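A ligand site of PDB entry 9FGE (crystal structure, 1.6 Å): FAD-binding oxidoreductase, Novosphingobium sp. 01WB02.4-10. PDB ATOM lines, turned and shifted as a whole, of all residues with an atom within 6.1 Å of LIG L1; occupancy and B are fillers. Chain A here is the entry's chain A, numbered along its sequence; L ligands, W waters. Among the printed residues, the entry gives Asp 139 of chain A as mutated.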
ATOM      1  N   TYR A  80      19.702 -19.275  14.838  1.00  0.00           N
ATOM      2  CA  TYR A  80      19.092 -18.047  14.346  1.00  0.00           C
ATOM      3  C   TYR A  80      20.109 -17.138  13.658  1.00  0.00           C
ATOM      4  O   TYR A  80      19.764 -16.018  13.268  1.00  0.00           O
ATOM      5  CB  TYR A  80      18.460 -17.283  15.518  1.00  0.00           C
ATOM      6  CG  TYR A  80      17.175 -17.820  16.093  1.00  0.00           C
ATOM      7  CD1 TYR A  80      16.084 -18.120  15.310  1.00  0.00           C
ATOM      8  CD2 TYR A  80      17.089 -18.111  17.452  1.00  0.00           C
ATOM      9  CE1 TYR A  80      14.916 -18.613  15.891  1.00  0.00           C
ATOM     10  CE2 TYR A  80      15.928 -18.582  18.054  1.00  0.00           C
ATOM     11  CZ  TYR A  80      14.825 -18.832  17.255  1.00  0.00           C
ATOM     12  OH  TYR A  80      13.636 -19.327  17.788  1.00  0.00           O
ATOM     13  N   ASP A 139      17.455 -22.395  27.570  1.00  0.00           N
ATOM     14  CA  ASP A 139      18.133 -23.683  27.581  1.00  0.00           C
ATOM     15  C   ASP A 139      19.389 -23.665  26.704  1.00  0.00           C
ATOM     16  O   ASP A 139      19.528 -24.426  25.776  1.00  0.00           O
ATOM     17  CB  ASP A 139      17.157 -24.743  27.091  1.00  0.00           C
ATOM     18  CG  ASP A 139      17.603 -26.172  27.366  1.00  0.00           C
ATOM     19  OD1 ASP A 139      18.617 -26.331  28.026  1.00  0.00           O
ATOM     20  OD2 ASP A 139      16.914 -27.066  26.863  1.00  0.00           O
ATOM     21  N   GLY A 154      13.329 -13.632  23.852  1.00  0.00           N
ATOM     22  CA  GLY A 154      13.438 -15.042  24.208  1.00  0.00           C
ATOM     23  C   GLY A 154      12.759 -15.389  25.518  1.00  0.00           C
ATOM     24  O   GLY A 154      12.065 -14.601  26.185  1.00  0.00           O
ATOM     25  N   VAL A 155      12.917 -16.680  25.842  1.00  0.00           N
ATOM     26  CA  VAL A 155      12.067 -17.363  26.782  1.00  0.00           C
ATOM     27  C   VAL A 155      12.875 -18.298  27.686  1.00  0.00           C
ATOM     28  O   VAL A 155      13.799 -18.955  27.188  1.00  0.00           O
ATOM     29  CB  VAL A 155      11.013 -18.155  25.994  1.00  0.00           C
ATOM     30  CG1 VAL A 155      10.207 -19.044  26.925  1.00  0.00           C
ATOM     31  CG2 VAL A 155      10.104 -17.182  25.223  1.00  0.00           C
ATOM     32  N   TYR A 157      12.152 -20.599  31.830  1.00  0.00           N
ATOM     33  CA  TYR A 157      11.278 -21.656  32.334  1.00  0.00           C
ATOM     34  C   TYR A 157      10.926 -21.497  33.820  1.00  0.00           C
ATOM     35  O   TYR A 157      10.528 -22.501  34.427  1.00  0.00           O
ATOM     36  CB  TYR A 157      11.850 -23.027  31.937  1.00  0.00           C
ATOM     37  CG  TYR A 157      12.068 -23.063  30.457  1.00  0.00           C
ATOM     38  CD1 TYR A 157      10.996 -22.922  29.603  1.00  0.00           C
ATOM     39  CD2 TYR A 157      13.337 -22.973  29.897  1.00  0.00           C
ATOM     40  CE1 TYR A 157      11.148 -22.710  28.240  1.00  0.00           C
ATOM     41  CE2 TYR A 157      13.508 -22.815  28.522  1.00  0.00           C
ATOM     42  CZ  TYR A 157      12.409 -22.690  27.686  1.00  0.00           C
ATOM     43  OH  TYR A 157      12.591 -22.459  26.334  1.00  0.00           O
ATOM     44  N   CYS A 262       6.711 -21.003  32.343  1.00  0.00           N
ATOM     45  CA  CYS A 262       6.638 -21.486  30.990  1.00  0.00           C
ATOM     46  C   CYS A 262       6.985 -22.981  30.965  1.00  0.00           C
ATOM     47  O   CYS A 262       7.969 -23.404  31.599  1.00  0.00           O
ATOM     48  CB  CYS A 262       7.561 -20.641  30.113  1.00  0.00           C
ATOM     49  SG  CYS A 262       7.626 -21.216  28.408  1.00  0.00           S
ATOM     50  N   LEU A 264       7.920 -26.446  28.989  1.00  0.00           N
ATOM     51  CA  LEU A 264       8.386 -27.149  27.800  1.00  0.00           C
ATOM     52  C   LEU A 264       7.693 -28.511  27.726  1.00  0.00           C
ATOM     53  O   LEU A 264       7.833 -29.323  28.623  1.00  0.00           O
ATOM     54  CB  LEU A 264       9.907 -27.326  27.848  1.00  0.00           C
ATOM     55  CG  LEU A 264      10.718 -26.074  27.510  1.00  0.00           C
ATOM     56  CD1 LEU A 264      12.209 -26.305  27.704  1.00  0.00           C
ATOM     57  CD2 LEU A 264      10.431 -25.629  26.091  1.00  0.00           C
ATOM     58  N   MET A 266       8.045 -31.505  25.444  1.00  0.00           N
ATOM     59  CA  MET A 266       9.131 -31.948  24.614  1.00  0.00           C
ATOM     60  C   MET A 266       8.746 -33.225  23.854  1.00  0.00           C
ATOM     61  O   MET A 266       8.260 -34.183  24.458  1.00  0.00           O
ATOM     62  CB  MET A 266      10.314 -32.282  25.531  1.00  0.00           C
ATOM     63  CG  MET A 266      10.755 -31.197  26.457  1.00  0.00           C
ATOM     64  SD  MET A 266      11.466 -29.803  25.604  1.00  0.00           S
ATOM     65  CE  MET A 266      12.777 -30.628  24.718  1.00  0.00           C
ATOM     66  N   TYR A 270      13.156 -34.979  19.969  1.00  0.00           N
ATOM     67  CA  TYR A 270      14.039 -33.930  20.461  1.00  0.00           C
ATOM     68  C   TYR A 270      14.863 -34.373  21.667  1.00  0.00           C
ATOM     69  O   TYR A 270      16.082 -34.219  21.730  1.00  0.00           O
ATOM     70  CB  TYR A 270      13.252 -32.649  20.769  1.00  0.00           C
ATOM     71  CG  TYR A 270      14.115 -31.440  21.105  1.00  0.00           C
ATOM     72  CD1 TYR A 270      14.774 -31.319  22.322  1.00  0.00           C
ATOM     73  CD2 TYR A 270      14.257 -30.412  20.196  1.00  0.00           C
ATOM     74  CE1 TYR A 270      15.572 -30.228  22.621  1.00  0.00           C
ATOM     75  CE2 TYR A 270      15.058 -29.322  20.481  1.00  0.00           C
ATOM     76  CZ  TYR A 270      15.707 -29.222  21.691  1.00  0.00           C
ATOM     77  OH  TYR A 270      16.491 -28.109  22.057  1.00  0.00           O
ATOM     78  N   TRP A 378      16.042 -23.037  13.761  1.00  0.00           N
ATOM     79  CA  TRP A 378      14.747 -22.987  14.401  1.00  0.00           C
ATOM     80  C   TRP A 378      13.695 -22.391  13.475  1.00  0.00           C
ATOM     81  O   TRP A 378      13.930 -21.281  12.942  1.00  0.00           O
ATOM     82  CB  TRP A 378      14.795 -22.164  15.693  1.00  0.00           C
ATOM     83  CG  TRP A 378      15.864 -22.588  16.661  1.00  0.00           C
ATOM     84  CD1 TRP A 378      17.005 -21.927  16.995  1.00  0.00           C
ATOM     85  CD2 TRP A 378      15.823 -23.781  17.467  1.00  0.00           C
ATOM     86  NE1 TRP A 378      17.707 -22.640  17.914  1.00  0.00           N
ATOM     87  CE2 TRP A 378      17.012 -23.771  18.242  1.00  0.00           C
ATOM     88  CE3 TRP A 378      14.916 -24.826  17.598  1.00  0.00           C
ATOM     89  CZ2 TRP A 378      17.323 -24.792  19.116  1.00  0.00           C
ATOM     90  CZ3 TRP A 378      15.222 -25.822  18.504  1.00  0.00           C
ATOM     91  CH2 TRP A 378      16.385 -25.790  19.263  1.00  0.00           C
ATOM     92  N   ALA A 380       9.889 -21.293  14.320  1.00  0.00           N
ATOM     93  CA  ALA A 380       9.302 -21.007  15.634  1.00  0.00           C
ATOM     94  C   ALA A 380       7.935 -20.328  15.488  1.00  0.00           C
ATOM     95  O   ALA A 380       7.757 -19.201  15.997  1.00  0.00           O
ATOM     96  CB  ALA A 380      10.261 -20.213  16.473  1.00  0.00           C
ATOM     97  N   ALA A 411       9.542 -28.925  20.296  1.00  0.00           N
ATOM     98  CA  ALA A 411       8.910 -28.729  21.589  1.00  0.00           C
ATOM     99  C   ALA A 411       7.879 -27.616  21.467  1.00  0.00           C
ATOM    100  O   ALA A 411       8.007 -26.777  20.584  1.00  0.00           O
ATOM    101  CB  ALA A 411       9.943 -28.383  22.631  1.00  0.00           C
ATOM    102  N   ALA A 413       6.698 -24.491  23.858  1.00  0.00           N
ATOM    103  CA  ALA A 413       6.838 -23.709  25.052  1.00  0.00           C
ATOM    104  C   ALA A 413       5.478 -23.111  25.363  1.00  0.00           C
ATOM    105  O   ALA A 413       5.013 -22.198  24.657  1.00  0.00           O
ATOM    106  CB  ALA A 413       7.867 -22.590  24.875  1.00  0.00           C
ATOM    107  N   HIS A 420       4.676 -21.162  21.920  1.00  0.00           N
ATOM    108  CA  HIS A 420       5.740 -21.060  20.932  1.00  0.00           C
ATOM    109  C   HIS A 420       6.034 -22.490  20.463  1.00  0.00           C
ATOM    110  O   HIS A 420       6.522 -23.294  21.292  1.00  0.00           O
ATOM    111  CB  HIS A 420       7.032 -20.448  21.475  1.00  0.00           C
ATOM    112  CG  HIS A 420       6.988 -19.060  21.961  1.00  0.00           C
ATOM    113  ND1 HIS A 420       5.923 -18.536  22.692  1.00  0.00           N
ATOM    114  CD2 HIS A 420       7.901 -18.061  21.874  1.00  0.00           C
ATOM    115  CE1 HIS A 420       6.213 -17.240  22.996  1.00  0.00           C
ATOM    116  NE2 HIS A 420       7.434 -16.949  22.546  1.00  0.00           N
ATOM    117  N   ILE A 422       8.380 -24.721  18.873  1.00  0.00           N
ATOM    118  CA  ILE A 422       9.795 -24.651  18.516  1.00  0.00           C
ATOM    119  C   ILE A 422      10.233 -25.891  17.744  1.00  0.00           C
ATOM    120  O   ILE A 422      10.300 -26.976  18.314  1.00  0.00           O
ATOM    121  CB  ILE A 422      10.650 -24.450  19.769  1.00  0.00           C
ATOM    122  CG1 ILE A 422      10.163 -23.223  20.568  1.00  0.00           C
ATOM    123  CG2 ILE A 422      12.134 -24.373  19.427  1.00  0.00           C
ATOM    124  CD1 ILE A 422      10.204 -21.934  19.801  1.00  0.00           C
ATOM    125  N   TYR A 457       7.427 -16.250  15.851  1.00  0.00           N
ATOM    126  CA  TYR A 457       7.734 -15.266  16.905  1.00  0.00           C
ATOM    127  C   TYR A 457       9.121 -14.666  16.748  1.00  0.00           C
ATOM    128  O   TYR A 457       9.386 -13.608  17.316  1.00  0.00           O
ATOM    129  CB  TYR A 457       7.593 -15.845  18.330  1.00  0.00           C
ATOM    130  CG  TYR A 457       8.806 -16.362  19.094  1.00  0.00           C
ATOM    131  CD1 TYR A 457       9.391 -17.568  18.796  1.00  0.00           C
ATOM    132  CD2 TYR A 457       9.417 -15.558  20.057  1.00  0.00           C
ATOM    133  CE1 TYR A 457      10.535 -17.994  19.452  1.00  0.00           C
ATOM    134  CE2 TYR A 457      10.523 -15.984  20.741  1.00  0.00           C
ATOM    135  CZ  TYR A 457      11.099 -17.197  20.435  1.00  0.00           C
ATOM    136  OH  TYR A 457      12.240 -17.524  21.144  1.00  0.00           O
ATOM    137  N   ARG A 458      10.013 -15.363  16.021  1.00  0.00           N
ATOM    138  CA  ARG A 458      11.459 -15.146  15.982  1.00  0.00           C
ATOM    139  C   ARG A 458      11.963 -16.000  14.827  1.00  0.00           C
ATOM    140  O   ARG A 458      11.468 -17.114  14.593  1.00  0.00           O
ATOM    141  CB  ARG A 458      12.059 -15.557  17.316  1.00  0.00           C
ATOM    142  CG  ARG A 458      13.525 -15.213  17.587  1.00  0.00           C
ATOM    143  CD  ARG A 458      13.848 -15.643  18.991  1.00  0.00           C
ATOM    144  NE  ARG A 458      15.247 -15.407  19.327  1.00  0.00           N
ATOM    145  CZ  ARG A 458      15.770 -15.843  20.456  1.00  0.00           C
ATOM    146  NH1 ARG A 458      15.036 -16.520  21.304  1.00  0.00           N
ATOM    147  NH2 ARG A 458      17.020 -15.557  20.743  1.00  0.00           N
HETATM  148  C1  LIG L   1      14.313 -23.187  22.272  1.00  0.00           C
HETATM  149  C2  LIG L   1      13.251 -22.401  22.753  1.00  0.00           C
HETATM  150  C3  LIG L   1      12.960 -21.202  22.125  1.00  0.00           C
HETATM  151  C4  LIG L   1      13.652 -20.825  20.989  1.00  0.00           C
HETATM  152  C5  LIG L   1      14.653 -21.642  20.491  1.00  0.00           C
HETATM  153  O1  LIG L   1      14.149 -24.919  23.890  1.00  0.00           O
HETATM  154  C6  LIG L   1      15.011 -22.781  21.163  1.00  0.00           C
HETATM  155  C7  LIG L   1      14.682 -24.457  22.934  1.00  0.00           C
HETATM  156  C8  LIG L   1      11.080 -20.722  23.478  1.00  0.00           C
HETATM  157  O2  LIG L   1      11.968 -20.325  22.435  1.00  0.00           O
HETATM  158  O3  LIG L   1      13.347 -19.657  20.318  1.00  0.00           O
HETATM  159  P1  LG2 L   2      22.668 -12.213  21.113  1.00  0.00           P
HETATM  160  O1  LG2 L   2      22.998 -13.204  20.030  1.00  0.00           O
HETATM  161  O2  LG2 L   2      23.799 -11.324  21.578  1.00  0.00           O
HETATM  162  O3  LG2 L   2      21.455 -11.285  20.687  1.00  0.00           O
HETATM  163  C1  LG2 L   2      20.331 -11.718  19.905  1.00  0.00           C
HETATM  164  C2  LG2 L   2      19.961 -10.607  18.927  1.00  0.00           C
HETATM  165  O4  LG2 L   2      19.507  -9.408  19.620  1.00  0.00           O
HETATM  166  C3  LG2 L   2      21.110 -10.126  18.036  1.00  0.00           C
HETATM  167  O5  LG2 L   2      21.340 -10.992  16.944  1.00  0.00           O
HETATM  168  C4  LG2 L   2      20.658  -8.717  17.689  1.00  0.00           C
HETATM  169  O6  LG2 L   2      19.660  -8.698  16.692  1.00  0.00           O
HETATM  170  C5  LG2 L   2      20.007  -8.235  18.958  1.00  0.00           C
HETATM  171  N1  LG2 L   2      20.886  -7.560  19.873  1.00  0.00           N
HETATM  172  C6  LG2 L   2      21.691  -8.185  20.871  1.00  0.00           C
HETATM  173  N2  LG2 L   2      22.315  -7.301  21.637  1.00  0.00           N
HETATM  174  C7  LG2 L   2      21.838  -6.085  21.191  1.00  0.00           C
HETATM  175  C8  LG2 L   2      22.106  -4.774  21.635  1.00  0.00           C
HETATM  176  N3  LG2 L   2      22.883  -4.534  22.667  1.00  0.00           N
HETATM  177  N4  LG2 L   2      21.516  -3.727  20.986  1.00  0.00           N
HETATM  178  C9  LG2 L   2      20.666  -4.053  20.006  1.00  0.00           C
HETATM  179  N5  LG2 L   2      20.364  -5.242  19.452  1.00  0.00           N
HETATM  180  C10 LG2 L   2      21.040  -6.230  20.069  1.00  0.00           C
HETATM  181  N6  LG2 L   2      16.529 -19.232  23.112  1.00  0.00           N
HETATM  182  C11 LG2 L   2      15.575 -18.948  24.014  1.00  0.00           C
HETATM  183  O7  LG2 L   2      15.093 -17.791  24.078  1.00  0.00           O
HETATM  184  N7  LG2 L   2      15.048 -19.899  24.877  1.00  0.00           N
HETATM  185  C12 LG2 L   2      15.571 -21.178  24.940  1.00  0.00           C
HETATM  186  O8  LG2 L   2      15.139 -21.975  25.813  1.00  0.00           O
HETATM  187  C13 LG2 L   2      16.554 -21.507  23.984  1.00  0.00           C
HETATM  188  N8  LG2 L   2      17.070 -22.743  23.959  1.00  0.00           N
HETATM  189  C14 LG2 L   2      18.051 -23.018  23.034  1.00  0.00           C
HETATM  190  C15 LG2 L   2      18.503 -24.355  22.933  1.00  0.00           C
HETATM  191  C16 LG2 L   2      19.469 -24.718  22.037  1.00  0.00           C
HETATM  192  C17 LG2 L   2      19.927 -26.156  22.001  1.00  0.00           C
HETATM  193  C18 LG2 L   2      19.972 -23.752  21.151  1.00  0.00           C
HETATM  194  C19 LG2 L   2      21.018 -24.115  20.134  1.00  0.00           C
HETATM  195  C20 LG2 L   2      19.508 -22.441  21.201  1.00  0.00           C
HETATM  196  C21 LG2 L   2      18.528 -22.051  22.128  1.00  0.00           C
HETATM  197  N9  LG2 L   2      18.040 -20.746  22.231  1.00  0.00           N
HETATM  198  C22 LG2 L   2      16.996 -20.456  23.082  1.00  0.00           C
HETATM  199  C23 LG2 L   2      18.425 -19.736  21.211  1.00  0.00           C
HETATM  200  C24 LG2 L   2      19.616 -18.837  21.558  1.00  0.00           C
HETATM  201  O9  LG2 L   2      20.791 -19.639  21.675  1.00  0.00           O
HETATM  202  C25 LG2 L   2      19.390 -18.012  22.831  1.00  0.00           C
HETATM  203  O10 LG2 L   2      18.190 -17.280  22.702  1.00  0.00           O
HETATM  204  C26 LG2 L   2      20.544 -17.084  23.216  1.00  0.00           C
HETATM  205  O11 LG2 L   2      20.299 -16.545  24.541  1.00  0.00           O
HETATM  206  C27 LG2 L   2      20.717 -15.968  22.215  1.00  0.00           C
HETATM  207  O12 LG2 L   2      22.103 -15.526  22.129  1.00  0.00           O
HETATM  208  P2  LG2 L   2      22.637 -14.330  23.056  1.00  0.00           P
HETATM  209  O13 LG2 L   2      22.024 -14.373  24.425  1.00  0.00           O
HETATM  210  O14 LG2 L   2      24.132 -14.319  22.943  1.00  0.00           O
HETATM  211  O15 LG2 L   2      22.086 -12.995  22.403  1.00  0.00           O
HETATM  212  O   HOH W   1      15.007 -27.130  24.587  1.00  0.00           O
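The side-chain hydroxyl of Tyr 457 is in hydrogen-bond range of an oxygen (O3) of LIG L1, at 2.5 Å.
NH2 of Arg 458 sits at hydrogen-bond distance from O10 of LG2 L2, 2.9 Å away.
O3 of LIG L1 sits at hydrogen-bond distance from OH of Tyr 80, at 2.6 Å.
The backbone NH of Asp 139 sits at hydrogen-bond distance from an oxygen (O8) of LG2 L2.
An oxygen (O8) of LG2 L2 lies within hydrogen-bond range of the side-chain hydroxyl of Tyr 157, 2.6 Å away.
An oxygen (O7) of LG2 L2 is in hydrogen-bond range of the backbone NH (N) of Val 155 (3.0 Å).
The backbone carbonyl oxygen (O) of Val 155 lies within hydrogen-bond range of a nitrogen (N7) of LG2 L2 (2.8 Å).
N of Ile 422 sits at hydrogen-bond distance from O of Ala 411, 2.7 Å away.
O of Ala 380 sits at hydrogen-bond distance from N of Tyr 457 (3.0 Å).
N of Ala 413 is in hydrogen-bond range of O of His 420, 2.8 Å away.
The side-chain hydroxyl of Tyr 457 lies within hydrogen-bond range of the guanidinium group of Arg 458.
Val 155 touches LIG L1.
Tyr 157 touches LIG L1 (OH to C2, 3.6 Å).
CE2 of Trp 378 touches C6 of LIG L1 (3.7 Å).
Ala 413 touches LIG L1 (CB to C8, 3.97 Å).
Ile 422 touches LIG L1.
NH1 of Arg 458 touches O3 of LIG L1 (3.7 Å).
Hydrophobic or aromatic side chains that line LIG L1: Tyr 80, Val 155, Trp 378, Ala 413, Ile 422 and Tyr 457.
Eight residues have an atom within 4 Å of LIG L1: Tyr 80, Val 155, Tyr 157, Trp 378, Ala 413, Ile 422, Tyr 457 and Arg 458.
Along chain A the residues within 4 Å of LIG L1 span positions 80 to 458.
Water W1 lies within hydrogen-bond range of an oxygen (O1) of LIG L1, the side-chain carboxylate (OD2) of Asp 139 and the side-chain hydroxyl (OH) of Tyr 270.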
